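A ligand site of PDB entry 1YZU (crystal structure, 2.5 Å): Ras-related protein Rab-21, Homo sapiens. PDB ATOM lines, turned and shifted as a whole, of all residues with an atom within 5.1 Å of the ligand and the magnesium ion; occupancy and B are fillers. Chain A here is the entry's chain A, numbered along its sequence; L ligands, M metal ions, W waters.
The backbone NH (N) of Ala 150 is in hydrogen-bond range of an oxygen (O13) of the ligand (2.7 Å). ND1 of His 35 is in hydrogen-bond range of O8 of the ligand (3.1 Å). The side-chain amide nitrogen (ND2) of Asn 119 lies within hydrogen-bond range of a nitrogen (N3) of the ligand, 3.1 Å away. N of Ser 21 sits at hydrogen-bond distance from O7 of the ligand (2.8 Å). The side-chain carboxylate (OD2) of Asp 122 lies within hydrogen-bond range of a nitrogen (N5) of the ligand, at 2.6 Å. O of Gly 15 lies within hydrogen-bond range of N1 of the ligand, at 3.1 Å. N of Lys 19 is in hydrogen-bond range of O4 of the ligand (2.9 Å). An oxygen (O3) of the ligand is in salt-bridge range of the side-chain amino group (NZ) of Lys 19 (2.7 Å). An oxygen (O2) of the ligand lies close to the backbone NH (N) of Thr 38 (3.3 Å). OG of Ser 149 is in hydrogen-bond range of O13 of the ligand, at 3.4 Å. OG1 of Thr 37 is in hydrogen-bond range of O1 of the ligand (2.9 Å). An oxygen (O11) of the ligand lies within hydrogen-bond range of the backbone carbonyl oxygen of Asp 33. N of Thr 20 lies close to O5 of the ligand (3.2 Å). The side-chain amino group (NZ) of Lys 120 is in hydrogen-bond range of an oxygen (O10) of the ligand. The backbone NH (N) of Gly 18 is in hydrogen-bond range of an oxygen (O4) of the ligand, 3.0 Å away. The backbone carbonyl oxygen (O) of Asn 32 lies within hydrogen-bond range of an oxygen (O12) of the ligand, 2.7 Å away. O7 of the ligand is in hydrogen-bond range of OG of Ser 21 (2.7 Å). The backbone NH (N) of Lys 151 is in hydrogen-bond range of an oxygen (O13) of the ligand (3.3 Å).
The side-chain amino group (NZ) of Lys 120 is in hydrogen-bond range of the backbone carbonyl oxygen (O) of Cys 16. OD1 of Asp 33 is in salt-bridge range of NZ of Lys 151, at 3.1 Å. O of Thr 148 sits at hydrogen-bond distance from N of Lys 120 (2.8 Å). The side-chain amino group of Lys 19 lies within hydrogen-bond range of the backbone carbonyl oxygen of Gly 13, 3.1 Å away. N of Ala 150 lies within hydrogen-bond range of OD1 of Asn 119, 3.4 Å away. The backbone carbonyl oxygen of Glu 14 sits at hydrogen-bond distance from the side-chain amino group of Lys 19, 2.9 Å away. The side-chain amide oxygen (OD1) of Asn 119 lies within hydrogen-bond range of the side-chain hydroxyl (OG1) of Thr 148, at 2.9 Å. The backbone carbonyl oxygen (O) of Val 17 lies within hydrogen-bond range of the side-chain amide nitrogen (ND2) of Asn 119 (2.7 Å).
O10 of the ligand sits close to O of Cys 16, 3.5 Å away. Glu 14 touches the ligand (O to O4, 3.7 Å). Val 17 touches the ligand. CZ of Phe 31 touches O12 of the ligand, at 3.5 Å. CD1 of Leu 123 touches N5 of the ligand, at 3.4 Å. Within 4 Å of the ligand: Glu 14, Gly 15, Cys 16, Val 17, Gly 18, Lys 19, Thr 20, Ser 21, Phe 31, Asn 32, Asp 33, His 35, Thr 37, Thr 38, Asn 119, Lys 120, Asp 122, Leu 123, Ser 149, Ala 150 and Lys 151.
The nearest printed residue that does not touch the magnesium ion is Asp 61 (4.04 Å).
The magnesium ion is bound by an oxygen (O2) of the ligand (1.8 Å). The magnesium ion is bound by an oxygen (O5) of the ligand, 1.9 Å away. The magnesium ion is bound by water W6, at 2.0 Å. Water W4 binds the magnesium ion (2.1 Å). OG1 of Thr 38 binds the magnesium ion (2.1 Å). The magnesium ion is bound by OG1 of Thr 20, 2.2 Å away. The magnesium ion has six donor atoms within binding distance.
Water W6 bridges the side-chain carboxylate (OD1) of Asp 61 (2.6 Å) and the backbone carbonyl oxygen (O) of Thr 62 (3.1 Å). Water W4 bridges O of Ile 36 and O8 of the ligand. Water W1 lies within hydrogen-bond range of an oxygen (O3) of the ligand (2.6 Å) and the backbone NH (N) of Gly 15 (3.4 Å). Water W5 bridges O1 of the ligand (2.6 Å) and NE2 of His 35 (3.0 Å). Water W3 lies within hydrogen-bond range of O12 of the ligand (2.8 Å) and OD1 of Asp 33 (3.0 Å). Water W8 lies within hydrogen-bond range of O of Lys 34 (2.6 Å), N of Ile 36 (2.9 Å) and O8 of the ligand (3.2 Å).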
ATOM      1  N   GLY A  13     -19.919  -7.609 -21.731  1.00  0.00           N
ATOM      2  CA  GLY A  13     -18.948  -7.401 -22.803  1.00  0.00           C
ATOM      3  C   GLY A  13     -19.500  -7.891 -24.120  1.00  0.00           C
ATOM      4  O   GLY A  13     -20.555  -8.525 -24.166  1.00  0.00           O
ATOM      5  N   GLU A  14     -18.780  -7.646 -25.203  1.00  0.00           N
ATOM      6  CA  GLU A  14     -19.231  -8.022 -26.557  1.00  0.00           C
ATOM      7  C   GLU A  14     -19.054  -9.525 -26.829  1.00  0.00           C
ATOM      8  O   GLU A  14     -18.429 -10.223 -26.057  1.00  0.00           O
ATOM      9  CB  GLU A  14     -18.443  -7.224 -27.600  1.00  0.00           C
ATOM     10  CG  GLU A  14     -18.516  -5.715 -27.365  1.00  0.00           C
ATOM     11  CD  GLU A  14     -19.879  -5.160 -27.645  1.00  0.00           C
ATOM     12  OE1 GLU A  14     -20.222  -5.113 -28.840  1.00  0.00           O
ATOM     13  OE2 GLU A  14     -20.582  -4.769 -26.689  1.00  0.00           O
ATOM     14  N   GLY A  15     -19.606  -9.991 -27.947  1.00  0.00           N
ATOM     15  CA  GLY A  15     -19.505 -11.386 -28.349  1.00  0.00           C
ATOM     16  C   GLY A  15     -18.102 -11.965 -28.279  1.00  0.00           C
ATOM     17  O   GLY A  15     -17.720 -12.563 -27.265  1.00  0.00           O
ATOM     18  N   CYS A  16     -17.300 -11.775 -29.305  1.00  0.00           N
ATOM     19  CA  CYS A  16     -15.974 -12.374 -29.369  1.00  0.00           C
ATOM     20  C   CYS A  16     -15.179 -12.530 -28.054  1.00  0.00           C
ATOM     21  O   CYS A  16     -14.193 -13.275 -28.041  1.00  0.00           O
ATOM     22  CB  CYS A  16     -15.120 -11.603 -30.398  1.00  0.00           C
ATOM     23  SG  CYS A  16     -14.373  -9.971 -29.872  1.00  0.00           S
ATOM     24  N   VAL A  17     -15.601 -11.881 -26.970  1.00  0.00           N
ATOM     25  CA  VAL A  17     -14.684 -11.667 -25.830  1.00  0.00           C
ATOM     26  C   VAL A  17     -14.355 -12.851 -24.929  1.00  0.00           C
ATOM     27  O   VAL A  17     -13.232 -12.959 -24.411  1.00  0.00           O
ATOM     28  CB  VAL A  17     -15.141 -10.460 -24.932  1.00  0.00           C
ATOM     29  CG1 VAL A  17     -15.361  -9.202 -25.775  1.00  0.00           C
ATOM     30  CG2 VAL A  17     -16.369 -10.797 -24.119  1.00  0.00           C
ATOM     31  N   GLY A  18     -15.327 -13.745 -24.703  1.00  0.00           N
ATOM     32  CA  GLY A  18     -15.073 -14.923 -23.855  1.00  0.00           C
ATOM     33  C   GLY A  18     -15.748 -14.954 -22.502  1.00  0.00           C
ATOM     34  O   GLY A  18     -15.245 -15.592 -21.567  1.00  0.00           O
ATOM     35  N   LYS A  19     -16.905 -14.311 -22.379  1.00  0.00           N
ATOM     36  CA  LYS A  19     -17.609 -14.281 -21.092  1.00  0.00           C
ATOM     37  C   LYS A  19     -17.855 -15.723 -20.657  1.00  0.00           C
ATOM     38  O   LYS A  19     -17.449 -16.168 -19.574  1.00  0.00           O
ATOM     39  CB  LYS A  19     -18.948 -13.572 -21.232  1.00  0.00           C
ATOM     40  CG  LYS A  19     -18.894 -12.139 -21.728  1.00  0.00           C
ATOM     41  CD  LYS A  19     -20.299 -11.534 -21.825  1.00  0.00           C
ATOM     42  CE  LYS A  19     -21.031 -12.024 -23.062  1.00  0.00           C
ATOM     43  NZ  LYS A  19     -20.298 -11.604 -24.293  1.00  0.00           N
ATOM     44  N   THR A  20     -18.509 -16.464 -21.535  1.00  0.00           N
ATOM     45  CA  THR A  20     -18.868 -17.838 -21.294  1.00  0.00           C
ATOM     46  C   THR A  20     -17.604 -18.636 -21.015  1.00  0.00           C
ATOM     47  O   THR A  20     -17.538 -19.387 -20.043  1.00  0.00           O
ATOM     48  CB  THR A  20     -19.688 -18.409 -22.520  1.00  0.00           C
ATOM     49  OG1 THR A  20     -20.967 -17.767 -22.568  1.00  0.00           O
ATOM     50  CG2 THR A  20     -19.880 -19.954 -22.461  1.00  0.00           C
ATOM     51  N   SER A  21     -16.591 -18.456 -21.844  1.00  0.00           N
ATOM     52  CA  SER A  21     -15.359 -19.200 -21.652  1.00  0.00           C
ATOM     53  C   SER A  21     -14.742 -18.952 -20.268  1.00  0.00           C
ATOM     54  O   SER A  21     -14.238 -19.865 -19.614  1.00  0.00           O
ATOM     55  CB  SER A  21     -14.367 -18.896 -22.755  1.00  0.00           C
ATOM     56  OG  SER A  21     -14.943 -19.230 -23.996  1.00  0.00           O
ATOM     57  N   PHE A  31     -13.276 -25.959 -21.671  1.00  0.00           N
ATOM     58  CA  PHE A  31     -13.096 -24.919 -22.674  1.00  0.00           C
ATOM     59  C   PHE A  31     -13.444 -25.443 -24.068  1.00  0.00           C
ATOM     60  O   PHE A  31     -13.257 -26.627 -24.351  1.00  0.00           O
ATOM     61  CB  PHE A  31     -11.664 -24.389 -22.632  1.00  0.00           C
ATOM     62  CG  PHE A  31     -11.344 -23.369 -23.694  1.00  0.00           C
ATOM     63  CD1 PHE A  31     -11.563 -22.016 -23.475  1.00  0.00           C
ATOM     64  CD2 PHE A  31     -10.806 -23.782 -24.909  1.00  0.00           C
ATOM     65  CE1 PHE A  31     -11.271 -21.091 -24.450  1.00  0.00           C
ATOM     66  CE2 PHE A  31     -10.524 -22.867 -25.893  1.00  0.00           C
ATOM     67  CZ  PHE A  31     -10.757 -21.503 -25.662  1.00  0.00           C
ATOM     68  N   ASN A  32     -13.971 -24.553 -24.919  1.00  0.00           N
ATOM     69  CA  ASN A  32     -14.304 -24.891 -26.298  1.00  0.00           C
ATOM     70  C   ASN A  32     -13.708 -23.840 -27.222  1.00  0.00           C
ATOM     71  O   ASN A  32     -13.806 -22.647 -26.925  1.00  0.00           O
ATOM     72  CB  ASN A  32     -15.822 -24.955 -26.462  1.00  0.00           C
ATOM     73  CG  ASN A  32     -16.456 -26.076 -25.621  1.00  0.00           C
ATOM     74  OD1 ASN A  32     -16.030 -27.233 -25.694  1.00  0.00           O
ATOM     75  ND2 ASN A  32     -17.487 -25.720 -24.819  1.00  0.00           N
ATOM     76  N   ASP A  33     -13.070 -24.259 -28.316  1.00  0.00           N
ATOM     77  CA  ASP A  33     -12.716 -23.310 -29.400  1.00  0.00           C
ATOM     78  C   ASP A  33     -13.964 -22.832 -30.132  1.00  0.00           C
ATOM     79  O   ASP A  33     -14.014 -21.693 -30.581  1.00  0.00           O
ATOM     80  CB  ASP A  33     -11.709 -23.888 -30.401  1.00  0.00           C
ATOM     81  CG  ASP A  33     -10.288 -23.871 -29.845  1.00  0.00           C
ATOM     82  OD1 ASP A  33      -9.957 -22.948 -29.092  1.00  0.00           O
ATOM     83  OD2 ASP A  33      -9.525 -24.798 -30.122  1.00  0.00           O
ATOM     84  N   LYS A  34     -14.983 -23.687 -30.226  1.00  0.00           N
ATOM     85  CA  LYS A  34     -16.221 -23.246 -30.817  1.00  0.00           C
ATOM     86  C   LYS A  34     -16.868 -22.102 -29.999  1.00  0.00           C
ATOM     87  O   LYS A  34     -16.918 -22.139 -28.757  1.00  0.00           O
ATOM     88  CB  LYS A  34     -17.227 -24.377 -31.011  1.00  0.00           C
ATOM     89  CG  LYS A  34     -18.453 -23.912 -31.751  1.00  0.00           C
ATOM     90  CD  LYS A  34     -19.096 -24.972 -32.659  1.00  0.00           C
ATOM     91  CE  LYS A  34     -20.602 -24.711 -32.811  1.00  0.00           C
ATOM     92  NZ  LYS A  34     -21.145 -25.101 -34.130  1.00  0.00           N
ATOM     93  N   HIS A  35     -17.373 -21.114 -30.740  1.00  0.00           N
ATOM     94  CA  HIS A  35     -18.193 -20.052 -30.224  1.00  0.00           C
ATOM     95  C   HIS A  35     -19.626 -20.569 -30.167  1.00  0.00           C
ATOM     96  O   HIS A  35     -20.270 -20.688 -31.191  1.00  0.00           O
ATOM     97  CB  HIS A  35     -18.082 -18.832 -31.144  1.00  0.00           C
ATOM     98  CG  HIS A  35     -19.028 -17.727 -30.812  1.00  0.00           C
ATOM     99  ND1 HIS A  35     -19.230 -17.276 -29.524  1.00  0.00           N
ATOM    100  CD2 HIS A  35     -19.809 -16.960 -31.604  1.00  0.00           C
ATOM    101  CE1 HIS A  35     -20.123 -16.307 -29.539  1.00  0.00           C
ATOM    102  NE2 HIS A  35     -20.493 -16.090 -30.785  1.00  0.00           N
ATOM    103  N   ILE A  36     -20.081 -20.910 -28.953  1.00  0.00           N
ATOM    104  CA  ILE A  36     -21.420 -21.453 -28.708  1.00  0.00           C
ATOM    105  C   ILE A  36     -22.196 -20.335 -28.040  1.00  0.00           C
ATOM    106  O   ILE A  36     -22.106 -20.125 -26.831  1.00  0.00           O
ATOM    107  CB  ILE A  36     -21.372 -22.694 -27.792  1.00  0.00           C
ATOM    108  CG1 ILE A  36     -20.581 -23.830 -28.457  1.00  0.00           C
ATOM    109  CG2 ILE A  36     -22.765 -23.203 -27.489  1.00  0.00           C
ATOM    110  CD1 ILE A  36     -20.115 -24.924 -27.474  1.00  0.00           C
ATOM    111  N   THR A  37     -22.925 -19.606 -28.864  1.00  0.00           N
ATOM    112  CA  THR A  37     -23.440 -18.288 -28.494  1.00  0.00           C
ATOM    113  C   THR A  37     -24.611 -18.423 -27.555  1.00  0.00           C
ATOM    114  O   THR A  37     -25.465 -19.319 -27.700  1.00  0.00           O
ATOM    115  CB  THR A  37     -23.821 -17.437 -29.747  1.00  0.00           C
ATOM    116  OG1 THR A  37     -23.968 -16.055 -29.377  1.00  0.00           O
ATOM    117  CG2 THR A  37     -25.086 -17.914 -30.361  1.00  0.00           C
ATOM    118  N   THR A  38     -24.615 -17.498 -26.600  1.00  0.00           N
ATOM    119  CA  THR A  38     -25.382 -17.589 -25.377  1.00  0.00           C
ATOM    120  C   THR A  38     -26.750 -16.932 -25.606  1.00  0.00           C
ATOM    121  O   THR A  38     -26.865 -15.708 -25.508  1.00  0.00           O
ATOM    122  CB  THR A  38     -24.582 -16.939 -24.223  1.00  0.00           C
ATOM    123  OG1 THR A  38     -23.264 -17.531 -24.175  1.00  0.00           O
ATOM    124  CG2 THR A  38     -25.287 -17.094 -22.863  1.00  0.00           C
ATOM    125  N   ASP A  61     -24.177 -15.185 -16.779  1.00  0.00           N
ATOM    126  CA  ASP A  61     -23.601 -15.018 -18.085  1.00  0.00           C
ATOM    127  C   ASP A  61     -24.755 -14.617 -19.003  1.00  0.00           C
ATOM    128  O   ASP A  61     -25.832 -15.200 -19.001  1.00  0.00           O
ATOM    129  CB  ASP A  61     -22.927 -16.308 -18.521  1.00  0.00           C
ATOM    130  CG  ASP A  61     -22.268 -16.208 -19.868  1.00  0.00           C
ATOM    131  OD1 ASP A  61     -22.056 -15.085 -20.360  1.00  0.00           O
ATOM    132  OD2 ASP A  61     -21.953 -17.268 -20.443  1.00  0.00           O
ATOM    133  N   THR A  62     -24.488 -13.614 -19.791  1.00  0.00           N
ATOM    134  CA  THR A  62     -25.537 -12.810 -20.353  1.00  0.00           C
ATOM    135  C   THR A  62     -25.669 -13.086 -21.837  1.00  0.00           C
ATOM    136  O   THR A  62     -24.726 -13.559 -22.467  1.00  0.00           O
ATOM    137  CB  THR A  62     -25.246 -11.346 -20.039  1.00  0.00           C
ATOM    138  OG1 THR A  62     -23.960 -10.993 -20.569  1.00  0.00           O
ATOM    139  CG2 THR A  62     -25.267 -11.140 -18.500  1.00  0.00           C
ATOM    140  N   ASN A 119      -9.338 -10.270 -21.680  1.00  0.00           N
ATOM    141  CA  ASN A 119      -9.238 -11.724 -21.887  1.00  0.00           C
ATOM    142  C   ASN A 119      -8.452 -12.036 -23.164  1.00  0.00           C
ATOM    143  O   ASN A 119      -8.287 -11.164 -24.036  1.00  0.00           O
ATOM    144  CB  ASN A 119     -10.646 -12.326 -21.931  1.00  0.00           C
ATOM    145  CG  ASN A 119     -10.668 -13.853 -21.988  1.00  0.00           C
ATOM    146  OD1 ASN A 119      -9.993 -14.540 -21.216  1.00  0.00           O
ATOM    147  ND2 ASN A 119     -11.487 -14.382 -22.893  1.00  0.00           N
ATOM    148  N   LYS A 120      -7.951 -13.272 -23.227  1.00  0.00           N
ATOM    149  CA  LYS A 120      -7.251 -13.843 -24.398  1.00  0.00           C
ATOM    150  C   LYS A 120      -5.791 -13.422 -24.430  1.00  0.00           C
ATOM    151  O   LYS A 120      -5.296 -13.005 -25.470  1.00  0.00           O
ATOM    152  CB  LYS A 120      -7.911 -13.499 -25.752  1.00  0.00           C
ATOM    153  CG  LYS A 120      -9.396 -13.758 -25.826  1.00  0.00           C
ATOM    154  CD  LYS A 120      -9.842 -13.819 -27.272  1.00  0.00           C
ATOM    155  CE  LYS A 120     -11.343 -13.875 -27.421  1.00  0.00           C
ATOM    156  NZ  LYS A 120     -11.768 -14.343 -28.765  1.00  0.00           N
ATOM    157  N   ILE A 121      -5.110 -13.542 -23.303  1.00  0.00           N
ATOM    158  CA  ILE A 121      -3.678 -13.167 -23.239  1.00  0.00           C
ATOM    159  C   ILE A 121      -2.771 -14.249 -23.822  1.00  0.00           C
ATOM    160  O   ILE A 121      -1.561 -14.059 -23.891  1.00  0.00           O
ATOM    161  CB  ILE A 121      -3.234 -12.813 -21.794  1.00  0.00           C
ATOM    162  CG1 ILE A 121      -3.287 -14.038 -20.874  1.00  0.00           C
ATOM    163  CG2 ILE A 121      -4.048 -11.615 -21.252  1.00  0.00           C
ATOM    164  CD1 ILE A 121      -2.921 -13.751 -19.432  1.00  0.00           C
ATOM    165  N   ASP A 122      -3.344 -15.373 -24.222  1.00  0.00           N
ATOM    166  CA  ASP A 122      -2.618 -16.381 -24.978  1.00  0.00           C
ATOM    167  C   ASP A 122      -2.358 -15.894 -26.407  1.00  0.00           C
ATOM    168  O   ASP A 122      -1.516 -16.443 -27.090  1.00  0.00           O
ATOM    169  CB  ASP A 122      -3.383 -17.718 -24.991  1.00  0.00           C
ATOM    170  CG  ASP A 122      -4.841 -17.570 -25.398  1.00  0.00           C
ATOM    171  OD1 ASP A 122      -5.628 -17.076 -24.560  1.00  0.00           O
ATOM    172  OD2 ASP A 122      -5.182 -17.928 -26.545  1.00  0.00           O
ATOM    173  N   LEU A 123      -3.082 -14.876 -26.838  1.00  0.00           N
ATOM    174  CA  LEU A 123      -2.899 -14.279 -28.162  1.00  0.00           C
ATOM    175  C   LEU A 123      -2.182 -12.928 -28.044  1.00  0.00           C
ATOM    176  O   LEU A 123      -2.561 -11.942 -28.716  1.00  0.00           O
ATOM    177  CB  LEU A 123      -4.275 -14.114 -28.834  1.00  0.00           C
ATOM    178  CG  LEU A 123      -5.172 -15.365 -28.855  1.00  0.00           C
ATOM    179  CD1 LEU A 123      -6.541 -15.036 -29.350  1.00  0.00           C
ATOM    180  CD2 LEU A 123      -4.549 -16.485 -29.705  1.00  0.00           C
ATOM    181  N   THR A 148      -6.724 -12.051 -18.361  1.00  0.00           N
ATOM    182  CA  THR A 148      -7.030 -13.496 -18.312  1.00  0.00           C
ATOM    183  C   THR A 148      -6.810 -14.229 -19.647  1.00  0.00           C
ATOM    184  O   THR A 148      -6.816 -13.617 -20.726  1.00  0.00           O
ATOM    185  CB  THR A 148      -8.522 -13.785 -17.887  1.00  0.00           C
ATOM    186  OG1 THR A 148      -9.411 -13.133 -18.787  1.00  0.00           O
ATOM    187  CG2 THR A 148      -8.808 -13.329 -16.501  1.00  0.00           C
ATOM    188  N   SER A 149      -6.596 -15.530 -19.528  1.00  0.00           N
ATOM    189  CA  SER A 149      -6.794 -16.457 -20.635  1.00  0.00           C
ATOM    190  C   SER A 149      -7.684 -17.593 -20.124  1.00  0.00           C
ATOM    191  O   SER A 149      -7.280 -18.346 -19.222  1.00  0.00           O
ATOM    192  CB  SER A 149      -5.481 -17.052 -21.130  1.00  0.00           C
ATOM    193  OG  SER A 149      -5.694 -17.754 -22.348  1.00  0.00           O
ATOM    194  N   ALA A 150      -8.885 -17.691 -20.702  1.00  0.00           N
ATOM    195  CA  ALA A 150      -9.774 -18.823 -20.441  1.00  0.00           C
ATOM    196  C   ALA A 150      -9.226 -20.113 -21.086  1.00  0.00           C
ATOM    197  O   ALA A 150      -9.325 -21.164 -20.498  1.00  0.00           O
ATOM    198  CB  ALA A 150     -11.178 -18.535 -20.938  1.00  0.00           C
ATOM    199  N   LYS A 151      -8.665 -20.006 -22.283  1.00  0.00           N
ATOM    200  CA  LYS A 151      -8.125 -21.140 -23.024  1.00  0.00           C
ATOM    201  C   LYS A 151      -6.963 -21.807 -22.282  1.00  0.00           C
ATOM    202  O   LYS A 151      -6.882 -23.046 -22.207  1.00  0.00           O
ATOM    203  CB  LYS A 151      -7.645 -20.669 -24.392  1.00  0.00           C
ATOM    204  CG  LYS A 151      -7.134 -21.787 -25.294  1.00  0.00           C
ATOM    205  CD  LYS A 151      -7.280 -21.391 -26.781  1.00  0.00           C
ATOM    206  CE  LYS A 151      -6.613 -22.403 -27.696  1.00  0.00           C
ATOM    207  NZ  LYS A 151      -6.974 -22.163 -29.129  1.00  0.00           N
HETATM  208  P1  LIG L   1     -21.463 -14.502 -26.592  1.00  0.00           P
HETATM  209  O1  LIG L   1     -21.963 -14.500 -28.031  1.00  0.00           O
HETATM  210  O2  LIG L   1     -22.085 -15.546 -25.681  1.00  0.00           O
HETATM  211  O3  LIG L   1     -21.661 -13.057 -26.083  1.00  0.00           O
HETATM  212  N1  LIG L   1     -19.868 -14.646 -26.612  1.00  0.00           N
HETATM  213  P2  LIG L   1     -18.919 -14.948 -25.367  1.00  0.00           P
HETATM  214  O4  LIG L   1     -18.342 -13.706 -24.791  1.00  0.00           O
HETATM  215  O5  LIG L   1     -19.714 -15.774 -24.443  1.00  0.00           O
HETATM  216  O6  LIG L   1     -17.695 -15.680 -25.976  1.00  0.00           O
HETATM  217  P3  LIG L   1     -17.249 -17.162 -25.918  1.00  0.00           P
HETATM  218  O7  LIG L   1     -16.945 -17.561 -24.516  1.00  0.00           O
HETATM  219  O8  LIG L   1     -18.193 -18.016 -26.660  1.00  0.00           O
HETATM  220  O9  LIG L   1     -15.899 -17.208 -26.724  1.00  0.00           O
HETATM  221  C1  LIG L   1     -15.956 -16.728 -28.083  1.00  0.00           C
HETATM  222  C2  LIG L   1     -14.744 -17.152 -28.892  1.00  0.00           C
HETATM  223  O10 LIG L   1     -13.586 -16.669 -28.177  1.00  0.00           O
HETATM  224  C3  LIG L   1     -14.587 -18.662 -29.015  1.00  0.00           C
HETATM  225  O11 LIG L   1     -13.938 -19.071 -30.264  1.00  0.00           O
HETATM  226  C4  LIG L   1     -13.735 -18.970 -27.789  1.00  0.00           C
HETATM  227  O12 LIG L   1     -13.084 -20.205 -27.872  1.00  0.00           O
HETATM  228  C5  LIG L   1     -12.772 -17.780 -27.819  1.00  0.00           C
HETATM  229  N2  LIG L   1     -12.094 -17.521 -26.549  1.00  0.00           N
HETATM  230  C6  LIG L   1     -12.662 -17.283 -25.312  1.00  0.00           C
HETATM  231  N3  LIG L   1     -11.787 -17.110 -24.343  1.00  0.00           N
HETATM  232  C7  LIG L   1     -10.549 -17.239 -24.979  1.00  0.00           C
HETATM  233  C8  LIG L   1      -9.222 -17.140 -24.487  1.00  0.00           C
HETATM  234  O13 LIG L   1      -8.816 -16.926 -23.324  1.00  0.00           O
HETATM  235  N4  LIG L   1      -8.278 -17.377 -25.500  1.00  0.00           N
HETATM  236  C9  LIG L   1      -8.550 -17.588 -26.831  1.00  0.00           C
HETATM  237  N5  LIG L   1      -7.491 -17.764 -27.647  1.00  0.00           N
HETATM  238  N6  LIG L   1      -9.779 -17.667 -27.299  1.00  0.00           N
HETATM  239  C10 LIG L   1     -10.727 -17.494 -26.337  1.00  0.00           C
HETATM  240 MG    MG M   1     -21.447 -16.541 -24.382  1.00  0.00          MG
HETATM  241  O   HOH W   1     -22.728 -11.194 -27.502  1.00  0.00           O
HETATM  242  O   HOH W   2     -10.384 -16.407 -29.647  1.00  0.00           O
HETATM  243  O   HOH W   3     -10.965 -20.149 -29.670  1.00  0.00           O
HETATM  244  O   HOH W   4     -20.912 -18.190 -25.493  1.00  0.00           O
HETATM  245  O   HOH W   5     -21.819 -13.385 -30.385  1.00  0.00           O
HETATM  246  O   HOH W   6     -22.222 -15.288 -22.970  1.00  0.00           O
HETATM  247  O   HOH W   7     -11.966 -17.807 -31.294  1.00  0.00           O
HETATM  248  O   HOH W   8     -18.228 -21.184 -26.748  1.00  0.00           O
